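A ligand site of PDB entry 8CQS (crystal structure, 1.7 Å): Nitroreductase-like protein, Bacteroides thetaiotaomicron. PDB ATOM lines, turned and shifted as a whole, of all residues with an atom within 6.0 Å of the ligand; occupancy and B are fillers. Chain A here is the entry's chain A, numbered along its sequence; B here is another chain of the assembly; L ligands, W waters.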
ATOM      1  N   ARG A  35      22.104  -4.308 -36.528  1.00  0.00           N
ATOM      2  CA  ARG A  35      21.264  -5.211 -35.748  1.00  0.00           C
ATOM      3  C   ARG A  35      20.286  -4.393 -34.875  1.00  0.00           C
ATOM      4  O   ARG A  35      20.654  -3.487 -34.096  1.00  0.00           O
ATOM      5  CB  ARG A  35      22.188  -6.123 -34.925  1.00  0.00           C
ATOM      6  CG  ARG A  35      21.633  -7.479 -34.504  1.00  0.00           C
ATOM      7  CD  ARG A  35      20.395  -7.482 -33.611  1.00  0.00           C
ATOM      8  NE  ARG A  35      20.586  -6.589 -32.467  1.00  0.00           N
ATOM      9  CZ  ARG A  35      19.610  -6.040 -31.728  1.00  0.00           C
ATOM     10  NH1 ARG A  35      18.323  -6.366 -31.954  1.00  0.00           N
ATOM     11  NH2 ARG A  35      19.928  -5.265 -30.719  1.00  0.00           N
ATOM     12  N   GLN A  36      18.978  -4.679 -34.982  1.00  0.00           N
ATOM     13  CA  GLN A  36      17.920  -3.907 -34.345  1.00  0.00           C
ATOM     14  C   GLN A  36      16.636  -4.749 -34.425  1.00  0.00           C
ATOM     15  O   GLN A  36      16.504  -5.592 -35.303  1.00  0.00           O
ATOM     16  CB  GLN A  36      17.700  -2.544 -35.011  1.00  0.00           C
ATOM     17  CG  GLN A  36      17.207  -2.743 -36.418  1.00  0.00           C
ATOM     18  CD  GLN A  36      17.075  -1.470 -37.183  1.00  0.00           C
ATOM     19  OE1 GLN A  36      16.654  -0.474 -36.644  1.00  0.00           O
ATOM     20  NE2 GLN A  36      17.388  -1.547 -38.470  1.00  0.00           N
ATOM     21  N   SER A  37      15.727  -4.442 -33.494  1.00  0.00           N
ATOM     22  CA  SER A  37      14.346  -4.999 -33.476  1.00  0.00           C
ATOM     23  C   SER A  37      13.483  -4.155 -34.391  1.00  0.00           C
ATOM     24  O   SER A  37      13.478  -2.962 -34.266  1.00  0.00           O
ATOM     25  CB  SER A  37      13.734  -5.060 -32.107  1.00  0.00           C
ATOM     26  OG  SER A  37      14.352  -6.092 -31.357  1.00  0.00           O
ATOM     27  N   THR A  38      12.774  -4.784 -35.306  1.00  0.00           N
ATOM     28  CA  THR A  38      11.804  -4.163 -36.147  1.00  0.00           C
ATOM     29  C   THR A  38      10.485  -4.901 -36.031  1.00  0.00           C
ATOM     30  O   THR A  38      10.489  -6.140 -36.116  1.00  0.00           O
ATOM     31  CB  THR A  38      12.326  -4.151 -37.587  1.00  0.00           C
ATOM     32  OG1 THR A  38      13.638  -3.572 -37.593  1.00  0.00           O
ATOM     33  CG2 THR A  38      11.371  -3.419 -38.499  1.00  0.00           C
ATOM     34  N   ARG A  39       9.407  -4.085 -35.852  1.00  0.00           N
ATOM     35  CA  ARG A  39       8.098  -4.659 -35.545  1.00  0.00           C
ATOM     36  C   ARG A  39       7.079  -4.228 -36.596  1.00  0.00           C
ATOM     37  O   ARG A  39       5.886  -4.171 -36.291  1.00  0.00           O
ATOM     38  CB  ARG A  39       7.678  -4.211 -34.146  1.00  0.00           C
ATOM     39  CG  ARG A  39       8.553  -4.854 -33.074  1.00  0.00           C
ATOM     40  CD  ARG A  39       8.045  -4.458 -31.710  1.00  0.00           C
ATOM     41  NE  ARG A  39       8.896  -4.910 -30.621  1.00  0.00           N
ATOM     42  CZ  ARG A  39       9.974  -4.273 -30.162  1.00  0.00           C
ATOM     43  NH1 ARG A  39      10.527  -3.243 -30.779  1.00  0.00           N
ATOM     44  NH2 ARG A  39      10.595  -4.789 -29.121  1.00  0.00           N
ATOM     45  N   GLN A 116       0.235  -9.882 -29.554  1.00  0.00           N
ATOM     46  CA  GLN A 116       0.890  -8.786 -30.259  1.00  0.00           C
ATOM     47  C   GLN A 116       0.609  -8.870 -31.751  1.00  0.00           C
ATOM     48  O   GLN A 116       1.333  -9.543 -32.495  1.00  0.00           O
ATOM     49  CB  GLN A 116       2.411  -8.747 -29.998  1.00  0.00           C
ATOM     50  CG  GLN A 116       2.790  -8.562 -28.553  1.00  0.00           C
ATOM     51  CD  GLN A 116       4.284  -8.319 -28.415  1.00  0.00           C
ATOM     52  OE1 GLN A 116       5.093  -9.239 -28.459  1.00  0.00           O
ATOM     53  NE2 GLN A 116       4.705  -7.048 -28.359  1.00  0.00           N
ATOM     54  N   PHE A 118       1.153  -7.078 -34.399  1.00  0.00           N
ATOM     55  CA  PHE A 118       2.134  -6.844 -35.444  1.00  0.00           C
ATOM     56  C   PHE A 118       2.740  -8.143 -35.969  1.00  0.00           C
ATOM     57  O   PHE A 118       3.184  -8.202 -37.084  1.00  0.00           O
ATOM     58  CB  PHE A 118       3.232  -5.876 -34.993  1.00  0.00           C
ATOM     59  CG  PHE A 118       4.267  -6.487 -34.085  1.00  0.00           C
ATOM     60  CD1 PHE A 118       5.374  -7.143 -34.626  1.00  0.00           C
ATOM     61  CD2 PHE A 118       4.205  -6.304 -32.697  1.00  0.00           C
ATOM     62  CE1 PHE A 118       6.325  -7.701 -33.791  1.00  0.00           C
ATOM     63  CE2 PHE A 118       5.174  -6.854 -31.873  1.00  0.00           C
ATOM     64  CZ  PHE A 118       6.234  -7.522 -32.426  1.00  0.00           C
ATOM     65  N   VAL A 170      12.449  -9.319 -34.977  1.00  0.00           N
ATOM     66  CA  VAL A 170      12.513  -8.947 -33.564  1.00  0.00           C
ATOM     67  C   VAL A 170      12.556 -10.241 -32.777  1.00  0.00           C
ATOM     68  O   VAL A 170      11.760 -11.150 -33.057  1.00  0.00           O
ATOM     69  CB  VAL A 170      11.327  -8.065 -33.116  1.00  0.00           C
ATOM     70  CG1 VAL A 170       9.971  -8.698 -33.427  1.00  0.00           C
ATOM     71  CG2 VAL A 170      11.397  -7.800 -31.629  1.00  0.00           C
ATOM     72  N   PRO A 171      13.490 -10.431 -31.813  1.00  0.00           N
ATOM     73  CA  PRO A 171      13.389 -11.630 -30.969  1.00  0.00           C
ATOM     74  C   PRO A 171      12.254 -11.464 -29.958  1.00  0.00           C
ATOM     75  O   PRO A 171      12.030 -10.366 -29.417  1.00  0.00           O
ATOM     76  CB  PRO A 171      14.781 -11.632 -30.320  1.00  0.00           C
ATOM     77  CG  PRO A 171      15.179 -10.210 -30.296  1.00  0.00           C
ATOM     78  CD  PRO A 171      14.578  -9.537 -31.473  1.00  0.00           C
ATOM     79  N   ARG A 172      11.484 -12.556 -29.700  1.00  0.00           N
ATOM     80  CA  ARG A 172      10.369 -12.459 -28.777  1.00  0.00           C
ATOM     81  C   ARG A 172      10.324 -13.687 -27.852  1.00  0.00           C
ATOM     82  O   ARG A 172      10.648 -14.823 -28.273  1.00  0.00           O
ATOM     83  CB  ARG A 172       9.048 -12.415 -29.574  1.00  0.00           C
ATOM     84  CG  ARG A 172       8.969 -11.254 -30.574  1.00  0.00           C
ATOM     85  CD  ARG A 172       7.625 -11.269 -31.266  1.00  0.00           C
ATOM     86  NE  ARG A 172       6.494 -11.182 -30.356  1.00  0.00           N
ATOM     87  CZ  ARG A 172       5.498 -12.053 -30.256  1.00  0.00           C
ATOM     88  NH1 ARG A 172       5.511 -13.232 -30.879  1.00  0.00           N
ATOM     89  NH2 ARG A 172       4.492 -11.741 -29.464  1.00  0.00           N
ATOM     90  N   ALA A 173       9.907 -13.429 -26.633  1.00  0.00           N
ATOM     91  CA  ALA A 173       9.487 -14.508 -25.756  1.00  0.00           C
ATOM     92  C   ALA A 173       7.964 -14.653 -25.710  1.00  0.00           C
ATOM     93  O   ALA A 173       7.511 -15.736 -25.293  1.00  0.00           O
ATOM     94  CB  ALA A 173      10.138 -14.316 -24.415  1.00  0.00           C
ATOM     95  N   SER A 174       7.189 -13.586 -25.948  1.00  0.00           N
ATOM     96  CA  SER A 174       5.744 -13.677 -25.902  1.00  0.00           C
ATOM     97  C   SER A 174       5.241 -14.563 -27.033  1.00  0.00           C
ATOM     98  O   SER A 174       5.747 -14.499 -28.145  1.00  0.00           O
ATOM     99  CB  SER A 174       5.018 -12.355 -26.040  1.00  0.00           C
ATOM    100  OG  SER A 174       5.529 -11.504 -25.037  1.00  0.00           O
ATOM    101  N   MET A 175       4.272 -15.393 -26.699  1.00  0.00           N
ATOM    102  CA  MET A 175       3.583 -16.224 -27.672  1.00  0.00           C
ATOM    103  C   MET A 175       2.528 -17.012 -26.930  1.00  0.00           C
ATOM    104  O   MET A 175       2.575 -17.068 -25.708  1.00  0.00           O
ATOM    105  CB  MET A 175       4.519 -17.178 -28.449  1.00  0.00           C
ATOM    106  CG  MET A 175       5.511 -17.858 -27.594  1.00  0.00           C
ATOM    107  SD  MET A 175       6.706 -18.828 -28.578  1.00  0.00           S
ATOM    108  CE  MET A 175       8.035 -18.904 -27.363  1.00  0.00           C
ATOM    109  N   MET A 194      11.482 -19.005 -27.663  1.00  0.00           N
ATOM    110  CA  MET A 194      11.521 -17.724 -28.325  1.00  0.00           C
ATOM    111  C   MET A 194      10.939 -17.852 -29.730  1.00  0.00           C
ATOM    112  O   MET A 194      10.711 -18.973 -30.262  1.00  0.00           O
ATOM    113  CB  MET A 194      12.938 -17.158 -28.460  1.00  0.00           C
ATOM    114  CG  MET A 194      13.638 -16.900 -27.175  1.00  0.00           C
ATOM    115  SD  MET A 194      15.300 -16.156 -27.371  1.00  0.00           S
ATOM    116  CE  MET A 194      14.894 -14.594 -28.098  1.00  0.00           C
ATOM    117  N   ASN B  62      25.413   0.133 -30.657  1.00  0.00           N
ATOM    118  CA  ASN B  62      25.386   0.331 -32.105  1.00  0.00           C
ATOM    119  C   ASN B  62      24.479   1.496 -32.511  1.00  0.00           C
ATOM    120  O   ASN B  62      24.535   1.876 -33.645  1.00  0.00           O
ATOM    121  CB  ASN B  62      25.031  -0.943 -32.866  1.00  0.00           C
ATOM    122  CG  ASN B  62      23.683  -1.552 -32.511  1.00  0.00           C
ATOM    123  OD1 ASN B  62      22.914  -0.965 -31.725  1.00  0.00           O
ATOM    124  ND2 ASN B  62      23.334  -2.608 -33.233  1.00  0.00           N
ATOM    125  N   ARG B  63      23.692   2.089 -31.587  1.00  0.00           N
ATOM    126  CA  ARG B  63      22.810   3.214 -31.844  1.00  0.00           C
ATOM    127  C   ARG B  63      22.991   4.230 -30.721  1.00  0.00           C
ATOM    128  O   ARG B  63      22.460   4.081 -29.635  1.00  0.00           O
ATOM    129  CB  ARG B  63      21.363   2.741 -31.949  1.00  0.00           C
ATOM    130  CG  ARG B  63      21.074   2.080 -33.279  1.00  0.00           C
ATOM    131  CD  ARG B  63      19.903   1.103 -33.211  1.00  0.00           C
ATOM    132  NE  ARG B  63      20.240  -0.053 -32.358  1.00  0.00           N
ATOM    133  CZ  ARG B  63      19.404  -0.967 -31.889  1.00  0.00           C
ATOM    134  NH1 ARG B  63      18.093  -0.793 -32.036  1.00  0.00           N
ATOM    135  NH2 ARG B  63      19.930  -2.015 -31.254  1.00  0.00           N
ATOM    136  N   LYS B  68      21.155   1.908 -27.628  1.00  0.00           N
ATOM    137  CA  LYS B  68      20.865   0.487 -27.838  1.00  0.00           C
ATOM    138  C   LYS B  68      22.089  -0.289 -28.351  1.00  0.00           C
ATOM    139  O   LYS B  68      23.067   0.290 -28.832  1.00  0.00           O
ATOM    140  CB  LYS B  68      19.600   0.319 -28.677  1.00  0.00           C
ATOM    141  CG  LYS B  68      18.325   0.700 -27.913  1.00  0.00           C
ATOM    142  CD  LYS B  68      17.074   0.444 -28.789  1.00  0.00           C
ATOM    143  CE  LYS B  68      15.754   0.681 -28.069  1.00  0.00           C
ATOM    144  NZ  LYS B  68      14.701   1.056 -29.050  1.00  0.00           N
ATOM    145  N   ARG B  69      21.980  -1.623 -28.314  1.00  0.00           N
ATOM    146  CA  ARG B  69      23.183  -2.470 -28.326  1.00  0.00           C
ATOM    147  C   ARG B  69      23.209  -3.446 -29.500  1.00  0.00           C
ATOM    148  O   ARG B  69      22.154  -3.729 -30.092  1.00  0.00           O
ATOM    149  CB  ARG B  69      23.285  -3.250 -27.013  1.00  0.00           C
ATOM    150  CG  ARG B  69      23.052  -2.494 -25.718  1.00  0.00           C
ATOM    151  CD  ARG B  69      24.155  -1.529 -25.377  1.00  0.00           C
ATOM    152  NE  ARG B  69      25.188  -2.240 -24.713  1.00  0.00           N
ATOM    153  CZ  ARG B  69      25.245  -2.578 -23.401  1.00  0.00           C
ATOM    154  NH1 ARG B  69      24.457  -2.101 -22.457  1.00  0.00           N
ATOM    155  NH2 ARG B  69      26.245  -3.353 -23.053  1.00  0.00           N
ATOM    156  N   ALA B  71      23.487  -6.572 -29.068  1.00  0.00           N
ATOM    157  CA  ALA B  71      22.718  -7.664 -28.519  1.00  0.00           C
ATOM    158  C   ALA B  71      21.364  -7.158 -28.054  1.00  0.00           C
ATOM    159  O   ALA B  71      21.292  -6.225 -27.240  1.00  0.00           O
ATOM    160  CB  ALA B  71      23.491  -8.279 -27.378  1.00  0.00           C
ATOM    161  N   PRO B  72      20.243  -7.741 -28.530  1.00  0.00           N
ATOM    162  CA  PRO B  72      18.944  -7.380 -27.964  1.00  0.00           C
ATOM    163  C   PRO B  72      18.849  -7.940 -26.525  1.00  0.00           C
ATOM    164  O   PRO B  72      19.620  -8.839 -26.106  1.00  0.00           O
ATOM    165  CB  PRO B  72      17.961  -8.002 -28.978  1.00  0.00           C
ATOM    166  CG  PRO B  72      18.741  -9.298 -29.386  1.00  0.00           C
ATOM    167  CD  PRO B  72      20.176  -8.777 -29.586  1.00  0.00           C
ATOM    168  N   SER B  73      17.876  -7.426 -25.767  1.00  0.00           N
ATOM    169  CA  SER B  73      17.640  -7.836 -24.403  1.00  0.00           C
ATOM    170  C   SER B  73      16.184  -7.685 -24.081  1.00  0.00           C
ATOM    171  O   SER B  73      15.518  -6.778 -24.569  1.00  0.00           O
ATOM    172  CB  SER B  73      18.511  -7.066 -23.410  1.00  0.00           C
ATOM    173  OG  SER B  73      18.229  -5.686 -23.429  1.00  0.00           O
ATOM    174  N   ALA B  74      15.667  -8.598 -23.218  1.00  0.00           N
ATOM    175  CA  ALA B  74      14.293  -8.513 -22.826  1.00  0.00           C
ATOM    176  C   ALA B  74      13.989  -7.152 -22.229  1.00  0.00           C
ATOM    177  O   ALA B  74      14.760  -6.691 -21.383  1.00  0.00           O
ATOM    178  CB  ALA B  74      13.891  -9.640 -21.854  1.00  0.00           C
ATOM    179  N   MET B  75      12.918  -6.497 -22.676  1.00  0.00           N
ATOM    180  CA  MET B  75      12.478  -5.181 -22.196  1.00  0.00           C
ATOM    181  C   MET B  75      13.561  -4.101 -22.330  1.00  0.00           C
ATOM    182  O   MET B  75      13.500  -3.066 -21.666  1.00  0.00           O
ATOM    183  CB  MET B  75      12.010  -5.257 -20.738  1.00  0.00           C
ATOM    184  CG  MET B  75      11.002  -6.330 -20.441  1.00  0.00           C
ATOM    185  SD  MET B  75      10.501  -6.230 -18.636  1.00  0.00           S
ATOM    186  CE  MET B  75      10.803  -7.918 -18.138  1.00  0.00           C
ATOM    187  N   ASN B  76      14.546  -4.315 -23.210  1.00  0.00           N
ATOM    188  CA  ASN B  76      15.705  -3.410 -23.365  1.00  0.00           C
ATOM    189  C   ASN B  76      16.394  -3.183 -22.010  1.00  0.00           C
ATOM    190  O   ASN B  76      16.882  -2.086 -21.741  1.00  0.00           O
ATOM    191  CB  ASN B  76      15.301  -2.039 -23.919  1.00  0.00           C
ATOM    192  CG  ASN B  76      16.487  -1.258 -24.449  1.00  0.00           C
ATOM    193  OD1 ASN B  76      17.471  -1.837 -24.869  1.00  0.00           O
ATOM    194  ND2 ASN B  76      16.402   0.070 -24.436  1.00  0.00           N
ATOM    195  N   MET B 146      15.099 -15.226 -18.578  1.00  0.00           N
ATOM    196  CA  MET B 146      15.335 -14.152 -19.530  1.00  0.00           C
ATOM    197  C   MET B 146      16.812 -13.805 -19.533  1.00  0.00           C
ATOM    198  O   MET B 146      17.355 -13.558 -20.633  1.00  0.00           O
ATOM    199  CB  MET B 146      14.498 -12.905 -19.219  1.00  0.00           C
ATOM    200  CG  MET B 146      13.012 -13.059 -19.510  1.00  0.00           C
ATOM    201  SD  MET B 146      12.087 -11.442 -19.093  1.00  0.00           S
ATOM    202  CE  MET B 146      12.288 -11.417 -17.317  1.00  0.00           C
ATOM    203  N   MET B 149      18.522 -16.427 -21.665  1.00  0.00           N
ATOM    204  CA  MET B 149      18.335 -16.125 -23.079  1.00  0.00           C
ATOM    205  C   MET B 149      19.271 -15.008 -23.510  1.00  0.00           C
ATOM    206  O   MET B 149      19.968 -15.148 -24.510  1.00  0.00           O
ATOM    207  CB  MET B 149      16.893 -15.722 -23.448  1.00  0.00           C
ATOM    208  CG  MET B 149      15.971 -16.841 -23.167  1.00  0.00           C
ATOM    209  SD  MET B 149      14.247 -16.320 -23.454  1.00  0.00           S
ATOM    210  CE  MET B 149      13.502 -17.936 -23.175  1.00  0.00           C
ATOM    211  N   ASP B 150      19.289 -13.929 -22.742  1.00  0.00           N
ATOM    212  CA  ASP B 150      20.055 -12.749 -23.026  1.00  0.00           C
ATOM    213  C   ASP B 150      21.546 -13.115 -23.098  1.00  0.00           C
ATOM    214  O   ASP B 150      22.300 -12.553 -23.939  1.00  0.00           O
ATOM    215  CB  ASP B 150      19.674 -11.637 -22.033  1.00  0.00           C
ATOM    216  CG  ASP B 150      18.377 -10.932 -22.342  1.00  0.00           C
ATOM    217  OD1 ASP B 150      17.679 -11.347 -23.266  1.00  0.00           O
ATOM    218  OD2 ASP B 150      18.012 -10.000 -21.554  1.00  0.00           O
ATOM    219  N   ILE B 153      22.308 -14.905 -26.338  1.00  0.00           N
ATOM    220  CA  ILE B 153      22.419 -13.927 -27.396  1.00  0.00           C
ATOM    221  C   ILE B 153      23.791 -13.275 -27.492  1.00  0.00           C
ATOM    222  O   ILE B 153      24.412 -13.222 -28.542  1.00  0.00           O
ATOM    223  CB  ILE B 153      21.268 -12.922 -27.192  1.00  0.00           C
ATOM    224  CG1 ILE B 153      19.931 -13.557 -27.509  1.00  0.00           C
ATOM    225  CG2 ILE B 153      21.492 -11.664 -27.993  1.00  0.00           C
ATOM    226  CD1 ILE B 153      18.766 -12.770 -27.073  1.00  0.00           C
HETATM  227  N1  LIG L   1       9.919  -7.706 -28.135  1.00  0.00           N
HETATM  228  C1  LIG L   1       8.574  -7.799 -28.198  1.00  0.00           C
HETATM  229  O1  LIG L   1       7.919  -6.975 -28.859  1.00  0.00           O
HETATM  230  N2  LIG L   1       7.912  -8.877 -27.646  1.00  0.00           N
HETATM  231  C2  LIG L   1       8.543  -9.805 -26.877  1.00  0.00           C
HETATM  232  O2  LIG L   1       7.908 -10.728 -26.403  1.00  0.00           O
HETATM  233  C3  LIG L   1       9.951  -9.672 -26.692  1.00  0.00           C
HETATM  234  N3  LIG L   1      10.552 -10.611 -25.979  1.00  0.00           N
HETATM  235  C4  LIG L   1      11.926 -10.513 -25.955  1.00  0.00           C
HETATM  236  C5  LIG L   1      12.644 -11.517 -25.258  1.00  0.00           C
HETATM  237  C6  LIG L   1      14.007 -11.546 -25.276  1.00  0.00           C
HETATM  238  C7  LIG L   1      14.736 -12.661 -24.554  1.00  0.00           C
HETATM  239  C8  LIG L   1      14.713 -10.550 -25.965  1.00  0.00           C
HETATM  240  C9  LIG L   1      16.213 -10.570 -26.015  1.00  0.00           C
HETATM  241  C10 LIG L   1      14.037  -9.568 -26.628  1.00  0.00           C
HETATM  242  C11 LIG L   1      12.637  -9.521 -26.631  1.00  0.00           C
HETATM  243  N4  LIG L   1      11.929  -8.504 -27.266  1.00  0.00           N
HETATM  244  C12 LIG L   1      10.592  -8.593 -27.406  1.00  0.00           C
HETATM  245  C13 LIG L   1      12.689  -7.477 -27.993  1.00  0.00           C
HETATM  246  C14 LIG L   1      13.250  -6.399 -27.045  1.00  0.00           C
HETATM  247  O3  LIG L   1      12.173  -5.506 -26.619  1.00  0.00           O
HETATM  248  C15 LIG L   1      14.298  -5.560 -27.754  1.00  0.00           C
HETATM  249  O4  LIG L   1      15.437  -6.358 -28.040  1.00  0.00           O
HETATM  250  C16 LIG L   1      14.755  -4.332 -26.930  1.00  0.00           C
HETATM  251  O5  LIG L   1      13.631  -3.420 -26.815  1.00  0.00           O
HETATM  252  C17 LIG L   1      15.955  -3.617 -27.500  1.00  0.00           C
HETATM  253  O6  LIG L   1      15.714  -3.244 -28.899  1.00  0.00           O
HETATM  254  P1  LIG L   1      16.781  -3.657 -29.971  1.00  0.00           P
HETATM  255  O7  LIG L   1      18.217  -3.393 -29.533  1.00  0.00           O
HETATM  256  O8  LIG L   1      16.564  -5.153 -30.164  1.00  0.00           O
HETATM  257  O9  LIG L   1      16.423  -2.891 -31.195  1.00  0.00           O
HETATM  258  O   HOH W   1      12.538  -2.162 -28.974  1.00  0.00           O
HETATM  259  O   HOH W   2      11.665  -2.936 -24.994  1.00  0.00           O
HETATM  260  O   HOH W   3      14.280  -1.337 -30.977  1.00  0.00           O
HETATM  261  O   HOH W   4      19.434  -2.763 -27.158  1.00  0.00           O
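The backbone NH (N) of Ser 37 sits at hydrogen-bond distance from an oxygen (O9) of the ligand (2.9 Å).
OG of Ser 37 lies within hydrogen-bond range of O8 of the ligand, at 2.7 Å.
O8 of the ligand lies within salt-bridge range of NH1 of Arg 35, at 2.8 Å.
The guanidinium group (NH2) of Arg 63 of chain B lies within salt-bridge range of an oxygen (O7) of the ligand (2.8 Å).
O2 of the ligand sits at hydrogen-bond distance from N of Ser 174, 3.0 Å away.
The side-chain hydroxyl (OG) of Ser 174 is in hydrogen-bond range of an oxygen (O2) of the ligand, 2.9 Å away.
O1 of the ligand is in hydrogen-bond range of NE of Arg 39 (2.9 Å).
N2 of the ligand is in hydrogen-bond range of OE1 of Gln 116, 3.0 Å away.
A nitrogen (N3) of the ligand is in hydrogen-bond range of the backbone NH (N) of Ala 173, 3.0 Å away.
O of Ser 73 of chain B sits close to O4 of the ligand (3.5 Å).
The backbone carbonyl oxygen of Arg 35 sits at hydrogen-bond distance from the side-chain amide nitrogen of Asn 62 of chain B, at 2.9 Å.
The backbone carbonyl oxygen (O) of Arg 63 of chain B is in hydrogen-bond range of the backbone NH (N) of Lys 68 of chain B (3.2 Å).
NH2 of Arg 63 of chain B lies within hydrogen-bond range of O of Arg 69 of chain B, 3.0 Å away.
OD1 of Asn 62 of chain B is in hydrogen-bond range of NE of Arg 63 of chain B (2.9 Å).
The backbone carbonyl oxygen (O) of Ser 174 sits at hydrogen-bond distance from the guanidinium group (NH1) of Arg 172, 3.0 Å away.
NH2 of Arg 172 lies within hydrogen-bond range of OE1 of Gln 116, at 2.8 Å.
N of Ala 74 of chain B sits at hydrogen-bond distance from OD2 of Asp 150 of chain B, 3.2 Å away.
The backbone carbonyl oxygen (O) of Arg 69 of chain B lies close to the side-chain amide oxygen (OD1) of Asn 62 of chain B (3.3 Å).
The backbone carbonyl oxygen (O) of Pro 171 lies close to a nitrogen (N4) of the ligand (2.8 Å).
CA of Gln 36 touches O9 of the ligand, 3.6 Å away.
Phe 118 touches the ligand (CZ to O1, 3.98 Å).
CG2 of Val 170 touches N1 of the ligand, at 3.8 Å.
Arg 172 touches the ligand (CA to N3, 3.4 Å).
Lys 68 of chain B touches the ligand (CD to O6, 3.9 Å).
Arg 69 of chain B touches the ligand (O to O7, 3.99 Å).
Pro 72 of chain B touches the ligand.
Ala 74 of chain B touches the ligand (N to C9, 3.5 Å).
OD1 of Asn 76 of chain B touches C17 of the ligand (3.5 Å).
Met 149 of chain B touches the ligand.
OD1 of Asp 150 of chain B touches C9 of the ligand, at 3.2 Å.
CD1 of Ile 153 of chain B touches C9 of the ligand, 3.5 Å away.
Hydrophobic or aromatic side chains within 4 Å of the ligand: Phe 118, Val 170, Pro 171, Ala 173, Pro 72 of chain B, Ala 74 of chain B, Met 149 of chain B and Ile 153 of chain B.
Of the 28 residues printed, 21 come within 4 Å of the ligand.
Water W3 lies within hydrogen-bond range of O9 of the ligand and NZ of Lys 68 of chain B.
Water W1 bridges O5 of the ligand and NH1 of Arg 39.
Water W4 lies within hydrogen-bond range of an oxygen (O7) of the ligand (2.7 Å), the backbone NH (N) of Arg 69 of chain B (3.0 Å) and the side-chain amide oxygen (OD1) of Asn 76 of chain B (3.2 Å).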
